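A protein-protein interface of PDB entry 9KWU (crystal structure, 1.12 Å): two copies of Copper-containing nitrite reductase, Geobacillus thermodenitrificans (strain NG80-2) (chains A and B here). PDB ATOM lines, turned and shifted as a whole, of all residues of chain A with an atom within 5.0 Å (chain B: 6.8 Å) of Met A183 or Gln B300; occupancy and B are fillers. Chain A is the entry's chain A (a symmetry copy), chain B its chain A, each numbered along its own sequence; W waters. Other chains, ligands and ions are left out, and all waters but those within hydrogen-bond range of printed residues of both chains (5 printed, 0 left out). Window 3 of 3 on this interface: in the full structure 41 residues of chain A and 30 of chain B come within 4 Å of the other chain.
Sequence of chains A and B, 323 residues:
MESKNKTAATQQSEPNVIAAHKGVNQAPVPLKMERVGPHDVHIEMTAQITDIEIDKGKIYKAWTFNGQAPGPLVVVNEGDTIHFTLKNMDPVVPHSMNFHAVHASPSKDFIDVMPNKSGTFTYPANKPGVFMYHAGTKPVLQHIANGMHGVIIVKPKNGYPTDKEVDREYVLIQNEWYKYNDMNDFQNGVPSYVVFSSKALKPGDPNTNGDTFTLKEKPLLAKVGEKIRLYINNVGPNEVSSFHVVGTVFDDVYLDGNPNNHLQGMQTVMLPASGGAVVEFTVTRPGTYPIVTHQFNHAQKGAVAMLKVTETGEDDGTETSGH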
ATOM      1  N   PRO A 139      16.383 -25.321 -10.456  1.00  0.00           N
ATOM      2  CA  PRO A 139      15.131 -24.674 -10.870  1.00  0.00           C
ATOM      3  C   PRO A 139      14.009 -25.008  -9.886  1.00  0.00           C
ATOM      4  O   PRO A 139      13.720 -26.181  -9.616  1.00  0.00           O
ATOM      5  CB  PRO A 139      14.826 -25.305 -12.240  1.00  0.00           C
ATOM      6  CG  PRO A 139      15.900 -26.273 -12.525  1.00  0.00           C
ATOM      7  CD  PRO A 139      16.682 -26.512 -11.269  1.00  0.00           C
ATOM      8  N   LEU A 141      10.839 -24.836 -10.119  1.00  0.00           N
ATOM      9  CA  LEU A 141       9.786 -25.664 -10.703  1.00  0.00           C
ATOM     10  C   LEU A 141      10.088 -27.148 -10.552  1.00  0.00           C
ATOM     11  O   LEU A 141       9.186 -27.956 -10.296  1.00  0.00           O
ATOM     12  CB  LEU A 141       9.643 -25.323 -12.191  1.00  0.00           C
ATOM     13  CG  LEU A 141       8.708 -26.222 -13.007  1.00  0.00           C
ATOM     14  CD1 LEU A 141       7.270 -26.216 -12.522  1.00  0.00           C
ATOM     15  CD2 LEU A 141       8.776 -25.821 -14.478  1.00  0.00           C
ATOM     16  N   GLN A 142      11.346 -27.537 -10.761  1.00  0.00           N
ATOM     17  CA  GLN A 142      11.713 -28.947 -10.676  1.00  0.00           C
ATOM     18  C   GLN A 142      11.515 -29.487  -9.266  1.00  0.00           C
ATOM     19  O   GLN A 142      11.007 -30.601  -9.078  1.00  0.00           O
ATOM     20  CB  GLN A 142      13.164 -29.132 -11.122  1.00  0.00           C
ATOM     21  CG  GLN A 142      13.586 -30.571 -11.237  1.00  0.00           C
ATOM     22  CD  GLN A 142      14.966 -30.731 -11.829  1.00  0.00           C
ATOM     23  OE1 GLN A 142      15.749 -29.783 -11.863  1.00  0.00           O
ATOM     24  NE2 GLN A 142      15.278 -31.937 -12.283  1.00  0.00           N
ATOM     25  N   ASN A 181      10.097 -36.290 -13.265  1.00  0.00           N
ATOM     26  CA  ASN A 181      11.305 -35.478 -13.389  1.00  0.00           C
ATOM     27  C   ASN A 181      11.547 -34.971 -14.808  1.00  0.00           C
ATOM     28  O   ASN A 181      12.691 -34.926 -15.271  1.00  0.00           O
ATOM     29  CB  ASN A 181      12.545 -36.220 -12.867  1.00  0.00           C
ATOM     30  CG  ASN A 181      13.710 -35.281 -12.646  1.00  0.00           C
ATOM     31  OD1 ASN A 181      13.525 -34.168 -12.145  1.00  0.00           O
ATOM     32  ND2 ASN A 181      14.917 -35.725 -12.987  1.00  0.00           N
ATOM     33  N   ASP A 182      10.480 -34.563 -15.493  1.00  0.00           N
ATOM     34  CA  ASP A 182      10.526 -34.179 -16.907  1.00  0.00           C
ATOM     35  C   ASP A 182      10.292 -32.674 -17.009  1.00  0.00           C
ATOM     36  O   ASP A 182       9.148 -32.211 -16.977  1.00  0.00           O
ATOM     37  CB  ASP A 182       9.472 -34.990 -17.666  1.00  0.00           C
ATOM     38  CG  ASP A 182       9.379 -34.647 -19.145  1.00  0.00           C
ATOM     39  OD1 ASP A 182       9.941 -33.619 -19.577  1.00  0.00           O
ATOM     40  OD2 ASP A 182       8.701 -35.416 -19.865  1.00  0.00           O
ATOM     41  N   MET A 183      11.389 -31.911 -17.116  1.00  0.00           N
ATOM     42  CA  MET A 183      11.291 -30.450 -17.135  1.00  0.00           C
ATOM     43  C   MET A 183      10.500 -29.933 -18.323  1.00  0.00           C
ATOM     44  O   MET A 183       9.845 -28.888 -18.213  1.00  0.00           O
ATOM     45  CB  MET A 183      12.695 -29.846 -17.091  1.00  0.00           C
ATOM     46  CG  MET A 183      13.277 -29.679 -15.683  1.00  0.00           C
ATOM     47  SD  MET A 183      12.367 -28.471 -14.657  1.00  0.00           S
ATOM     48  CE  MET A 183      13.002 -26.931 -15.196  1.00  0.00           C
ATOM     49  N   ASN A 184      10.545 -30.614 -19.466  1.00  0.00           N
ATOM     50  CA  ASN A 184       9.718 -30.174 -20.582  1.00  0.00           C
ATOM     51  C   ASN A 184       8.245 -30.277 -20.229  1.00  0.00           C
ATOM     52  O   ASN A 184       7.462 -29.348 -20.473  1.00  0.00           O
ATOM     53  CB  ASN A 184      10.038 -30.972 -21.843  1.00  0.00           C
ATOM     54  CG  ASN A 184       9.218 -30.505 -23.001  1.00  0.00           C
ATOM     55  OD1 ASN A 184       9.275 -29.334 -23.376  1.00  0.00           O
ATOM     56  ND2 ASN A 184       8.393 -31.393 -23.535  1.00  0.00           N
ATOM     57  N   ASP A 185       7.844 -31.414 -19.664  1.00  0.00           N
ATOM     58  CA  ASP A 185       6.456 -31.593 -19.249  1.00  0.00           C
ATOM     59  C   ASP A 185       6.088 -30.607 -18.150  1.00  0.00           C
ATOM     60  O   ASP A 185       4.988 -30.041 -18.156  1.00  0.00           O
ATOM     61  CB  ASP A 185       6.233 -33.041 -18.794  1.00  0.00           C
ATOM     62  CG  ASP A 185       4.769 -33.419 -18.731  1.00  0.00           C
ATOM     63  OD1 ASP A 185       4.070 -33.255 -19.757  1.00  0.00           O
ATOM     64  OD2 ASP A 185       4.332 -33.903 -17.658  1.00  0.00           O
ATOM     65  N   PHE A 186       6.983 -30.413 -17.178  1.00  0.00           N
ATOM     66  CA  PHE A 186       6.686 -29.496 -16.084  1.00  0.00           C
ATOM     67  C   PHE A 186       6.359 -28.097 -16.602  1.00  0.00           C
ATOM     68  O   PHE A 186       5.500 -27.406 -16.043  1.00  0.00           O
ATOM     69  CB  PHE A 186       7.887 -29.367 -15.140  1.00  0.00           C
ATOM     70  CG  PHE A 186       8.255 -30.602 -14.343  1.00  0.00           C
ATOM     71  CD1 PHE A 186       7.478 -31.750 -14.308  1.00  0.00           C
ATOM     72  CD2 PHE A 186       9.427 -30.576 -13.589  1.00  0.00           C
ATOM     73  CE1 PHE A 186       7.862 -32.851 -13.531  1.00  0.00           C
ATOM     74  CE2 PHE A 186       9.815 -31.661 -12.822  1.00  0.00           C
ATOM     75  CZ  PHE A 186       9.019 -32.802 -12.776  1.00  0.00           C
ATOM     76  N   GLN A 187       7.089 -27.657 -17.644  1.00  0.00           N
ATOM     77  CA  GLN A 187       6.953 -26.311 -18.201  1.00  0.00           C
ATOM     78  C   GLN A 187       5.788 -26.184 -19.171  1.00  0.00           C
ATOM     79  O   GLN A 187       5.124 -25.139 -19.211  1.00  0.00           O
ATOM     80  CB  GLN A 187       8.226 -25.920 -18.969  1.00  0.00           C
ATOM     81  CG  GLN A 187       9.398 -25.609 -18.081  1.00  0.00           C
ATOM     82  CD  GLN A 187      10.664 -25.371 -18.871  1.00  0.00           C
ATOM     83  OE1 GLN A 187      10.865 -24.311 -19.463  1.00  0.00           O
ATOM     84  NE2 GLN A 187      11.543 -26.354 -18.860  1.00  0.00           N
ATOM     85  N   ASN A 188       5.577 -27.212 -19.994  1.00  0.00           N
ATOM     86  CA  ASN A 188       4.758 -27.110 -21.195  1.00  0.00           C
ATOM     87  C   ASN A 188       3.585 -28.077 -21.275  1.00  0.00           C
ATOM     88  O   ASN A 188       2.771 -27.948 -22.208  1.00  0.00           O
ATOM     89  CB  ASN A 188       5.648 -27.338 -22.427  1.00  0.00           C
ATOM     90  CG  ASN A 188       6.705 -26.275 -22.572  1.00  0.00           C
ATOM     91  OD1 ASN A 188       6.414 -25.084 -22.485  1.00  0.00           O
ATOM     92  ND2 ASN A 188       7.947 -26.694 -22.760  1.00  0.00           N
ATOM     93  N   VAL B 194       7.295 -16.039 -20.431  1.00  0.00           N
ATOM     94  CA  VAL B 194       6.479 -15.179 -19.579  1.00  0.00           C
ATOM     95  C   VAL B 194       7.474 -14.293 -18.845  1.00  0.00           C
ATOM     96  O   VAL B 194       8.523 -14.779 -18.411  1.00  0.00           O
ATOM     97  CB  VAL B 194       5.568 -15.984 -18.630  1.00  0.00           C
ATOM     98  CG1 VAL B 194       4.616 -15.045 -17.892  1.00  0.00           C
ATOM     99  CG2 VAL B 194       4.779 -17.036 -19.391  1.00  0.00           C
ATOM    100  N   THR B 293       5.666 -14.863 -10.682  1.00  0.00           N
ATOM    101  CA  THR B 293       4.370 -15.535 -10.686  1.00  0.00           C
ATOM    102  C   THR B 293       4.596 -16.954 -10.163  1.00  0.00           C
ATOM    103  O   THR B 293       5.518 -17.645 -10.608  1.00  0.00           O
ATOM    104  CB  THR B 293       3.666 -15.541 -12.049  1.00  0.00           C
ATOM    105  OG1 THR B 293       2.468 -16.334 -11.886  1.00  0.00           O
ATOM    106  CG2 THR B 293       4.529 -16.106 -13.160  1.00  0.00           C
ATOM    107  N   GLN B 295       2.827 -19.544 -10.534  1.00  0.00           N
ATOM    108  CA  GLN B 295       2.597 -20.563 -11.564  1.00  0.00           C
ATOM    109  C   GLN B 295       3.970 -20.857 -12.131  1.00  0.00           C
ATOM    110  O   GLN B 295       4.484 -20.104 -12.959  1.00  0.00           O
ATOM    111  CB  GLN B 295       1.590 -20.053 -12.587  1.00  0.00           C
ATOM    112  CG  GLN B 295       0.205 -19.899 -11.958  1.00  0.00           C
ATOM    113  CD  GLN B 295      -0.681 -18.883 -12.661  1.00  0.00           C
ATOM    114  OE1 GLN B 295      -1.171 -17.938 -12.038  1.00  0.00           O
ATOM    115  NE2 GLN B 295      -0.934 -19.097 -13.945  1.00  0.00           N
ATOM    116  N   PHE B 296       4.620 -21.903 -11.605  1.00  0.00           N
ATOM    117  CA  PHE B 296       6.071 -22.008 -11.756  1.00  0.00           C
ATOM    118  C   PHE B 296       6.503 -22.419 -13.155  1.00  0.00           C
ATOM    119  O   PHE B 296       7.675 -22.204 -13.498  1.00  0.00           O
ATOM    120  CB  PHE B 296       6.742 -22.828 -10.632  1.00  0.00           C
ATOM    121  CG  PHE B 296       7.501 -21.941  -9.681  1.00  0.00           C
ATOM    122  CD1 PHE B 296       8.775 -21.506 -10.007  1.00  0.00           C
ATOM    123  CD2 PHE B 296       6.890 -21.418  -8.552  1.00  0.00           C
ATOM    124  CE1 PHE B 296       9.435 -20.596  -9.209  1.00  0.00           C
ATOM    125  CE2 PHE B 296       7.556 -20.504  -7.738  1.00  0.00           C
ATOM    126  CZ  PHE B 296       8.832 -20.085  -8.078  1.00  0.00           C
ATOM    127  N   ASN B 297       5.589 -22.938 -13.985  1.00  0.00           N
ATOM    128  CA  ASN B 297       5.911 -23.133 -15.394  1.00  0.00           C
ATOM    129  C   ASN B 297       6.202 -21.786 -16.060  1.00  0.00           C
ATOM    130  O   ASN B 297       7.128 -21.672 -16.878  1.00  0.00           O
ATOM    131  CB  ASN B 297       4.802 -23.901 -16.131  1.00  0.00           C
ATOM    132  CG  ASN B 297       3.382 -23.335 -15.960  1.00  0.00           C
ATOM    133  OD1 ASN B 297       3.080 -22.514 -15.121  1.00  0.00           O
ATOM    134  ND2 ASN B 297       2.476 -23.866 -16.768  1.00  0.00           N
ATOM    135  N   HIS B 298       5.445 -20.744 -15.695  1.00  0.00           N
ATOM    136  CA  HIS B 298       5.666 -19.398 -16.227  1.00  0.00           C
ATOM    137  C   HIS B 298       6.929 -18.768 -15.645  1.00  0.00           C
ATOM    138  O   HIS B 298       7.699 -18.123 -16.370  1.00  0.00           O
ATOM    139  CB  HIS B 298       4.442 -18.541 -15.931  1.00  0.00           C
ATOM    140  CG  HIS B 298       3.194 -19.055 -16.560  1.00  0.00           C
ATOM    141  ND1 HIS B 298       1.944 -18.593 -16.208  1.00  0.00           N
ATOM    142  CD2 HIS B 298       3.005 -20.006 -17.508  1.00  0.00           C
ATOM    143  CE1 HIS B 298       1.037 -19.240 -16.921  1.00  0.00           C
ATOM    144  NE2 HIS B 298       1.653 -20.101 -17.722  1.00  0.00           N
ATOM    145  N   ALA B 299       7.166 -18.961 -14.339  1.00  0.00           N
ATOM    146  CA  ALA B 299       8.411 -18.483 -13.742  1.00  0.00           C
ATOM    147  C   ALA B 299       9.620 -19.097 -14.449  1.00  0.00           C
ATOM    148  O   ALA B 299      10.602 -18.398 -14.764  1.00  0.00           O
ATOM    149  CB  ALA B 299       8.428 -18.788 -12.240  1.00  0.00           C
ATOM    150  N   GLN B 300       9.570 -20.407 -14.711  1.00  0.00           N
ATOM    151  CA  GLN B 300      10.685 -21.077 -15.365  1.00  0.00           C
ATOM    152  C   GLN B 300      10.916 -20.525 -16.771  1.00  0.00           C
ATOM    153  O   GLN B 300      12.049 -20.516 -17.250  1.00  0.00           O
ATOM    154  CB  GLN B 300      10.427 -22.579 -15.405  1.00  0.00           C
ATOM    155  CG  GLN B 300      11.487 -23.392 -16.112  1.00  0.00           C
ATOM    156  CD  GLN B 300      12.854 -23.291 -15.470  1.00  0.00           C
ATOM    157  OE1 GLN B 300      12.992 -23.063 -14.262  1.00  0.00           O
ATOM    158  NE2 GLN B 300      13.888 -23.491 -16.284  1.00  0.00           N
ATOM    159  N   LYS B 301       9.857 -20.078 -17.443  1.00  0.00           N
ATOM    160  CA  LYS B 301       9.919 -19.527 -18.788  1.00  0.00           C
ATOM    161  C   LYS B 301      10.163 -18.027 -18.796  1.00  0.00           C
ATOM    162  O   LYS B 301      10.009 -17.389 -19.849  1.00  0.00           O
ATOM    163  CB  LYS B 301       8.684 -19.941 -19.596  1.00  0.00           C
ATOM    164  CG  LYS B 301       8.708 -21.458 -19.878  1.00  0.00           C
ATOM    165  CD  LYS B 301       7.689 -21.990 -20.869  1.00  0.00           C
ATOM    166  CE  LYS B 301       6.287 -22.014 -20.312  1.00  0.00           C
ATOM    167  NZ  LYS B 301       5.343 -22.678 -21.298  1.00  0.00           N
ATOM    168  N   GLY B 302      10.609 -17.469 -17.665  1.00  0.00           N
ATOM    169  CA  GLY B 302      11.149 -16.128 -17.645  1.00  0.00           C
ATOM    170  C   GLY B 302      10.652 -15.217 -16.543  1.00  0.00           C
ATOM    171  O   GLY B 302      11.287 -14.186 -16.278  1.00  0.00           O
ATOM    172  N   ALA B 303       9.534 -15.562 -15.901  1.00  0.00           N
ATOM    173  CA  ALA B 303       8.804 -14.599 -15.066  1.00  0.00           C
ATOM    174  C   ALA B 303       9.311 -14.606 -13.625  1.00  0.00           C
ATOM    175  O   ALA B 303       8.604 -14.952 -12.674  1.00  0.00           O
ATOM    176  CB  ALA B 303       7.305 -14.861 -15.147  1.00  0.00           C
ATOM    177  N   VAL B 304      10.570 -14.180 -13.493  1.00  0.00           N
ATOM    178  CA  VAL B 304      11.245 -13.944 -12.227  1.00  0.00           C
ATOM    179  C   VAL B 304      12.011 -12.632 -12.377  1.00  0.00           C
ATOM    180  O   VAL B 304      12.842 -12.491 -13.286  1.00  0.00           O
ATOM    181  CB  VAL B 304      12.210 -15.079 -11.818  1.00  0.00           C
ATOM    182  CG1 VAL B 304      12.899 -14.732 -10.496  1.00  0.00           C
ATOM    183  CG2 VAL B 304      11.491 -16.412 -11.736  1.00  0.00           C
HETATM  184  O   HOH W   1       2.929 -27.266 -17.323  1.00  0.00           O
HETATM  185  O   HOH W   2       2.163 -25.661 -19.529  1.00  0.00           O
HETATM  186  O   HOH W   3      13.432 -23.513 -19.250  1.00  0.00           O
HETATM  187  O   HOH W   4      11.617 -22.631 -11.843  1.00  0.00           O
HETATM  188  O   HOH W   5       2.951 -22.960 -19.938  1.00  0.00           O
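The backbone carbonyl oxygen (O) of Gln A187 lies within hydrogen-bond range of the side-chain amino group (NZ) of Lys B301, at 3.2 Å.
The side-chain amide oxygen (OD1) of Asn A188 is in hydrogen-bond range of the side-chain amino group (NZ) of Lys B301, at 2.9 Å.
Of the printed residues of chain B, Leu A141 touches Phe B296 (3.9 Å), Asn B297 (3.96 Å) and Gln B300 (3.8 Å).
Val B194 touches none of the printed residues of chain A.
Gln B295 touches none of the printed residues of chain A.
Printed residues of chain A within 4 Å of Lys B301: Gln A187 (3.2 Å) and Asn A188 (2.9 Å).
The nearest printed residue of chain B that does not touch Met A183 is Phe B296 (7.3 Å).
The nearest printed residue of chain B that does not touch Leu A141 is His B298 (6.2 Å).
No position is printed for both chains.
Of the 10 pairs that touch across the chains among the printed residues, none has its exchanged pair printed and touching as well.
Water W3 bridges OE1 of Gln A187 (2.7 Å) and NE2 of Gln B300 (3.0 Å).
Water W5 lies within hydrogen-bond range of NZ of Lys B301 (2.8 Å), O of Gln A187 (3.2 Å) and ND2 of Asn B297 (3.3 Å).
Water W4 lies within hydrogen-bond range of the side-chain amide oxygen (OE1) of Gln B300 and the backbone NH (N) of Leu A141.
Water W1 lies within hydrogen-bond range of O of Phe A186 (2.9 Å) and ND2 of Asn B297 (3.5 Å).
Water W2 lies within hydrogen-bond range of the backbone carbonyl oxygen (O) of Gln A187 (3.0 Å) and the side-chain amide nitrogen (ND2) of Asn B297 (3.3 Å).
Among the printed residues, merely in contact across the chains: Gln A187 with Asn B297 (3.3 Å), Gln A187 with Gln B300 (3.5 Å), Pro A139 with Gln B300 (3.5 Å), Phe A186 with Asn B297 (3.6 Å), Met A183 with Gln B300 (3.7 Å), Leu A141 with Gln B300 (3.8 Å), Leu A141 with Phe B296 (3.9 Å) and Leu A141 with Asn B297 (3.96 Å).
The backbone NH (N) of Val B194 is in hydrogen-bond range of the backbone carbonyl oxygen (O) of Lys B301, 3.1 Å away.
The side-chain amide nitrogen (NE2) of Gln A187 is in hydrogen-bond range of the backbone carbonyl oxygen (O) of Met A183, at 3.1 Å.
OD1 of Asn A184 is in hydrogen-bond range of ND2 of Asn A188 (3.0 Å).
Hydrophobic or aromatic side chains of chain A that line the printed part of chain B: Pro A139, Leu A141 and Met A183.
Of the 12 printed residues of chain B, 4 touch a printed residue of chain A.
Among the printed residues, 10 pairs touch across the chains.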
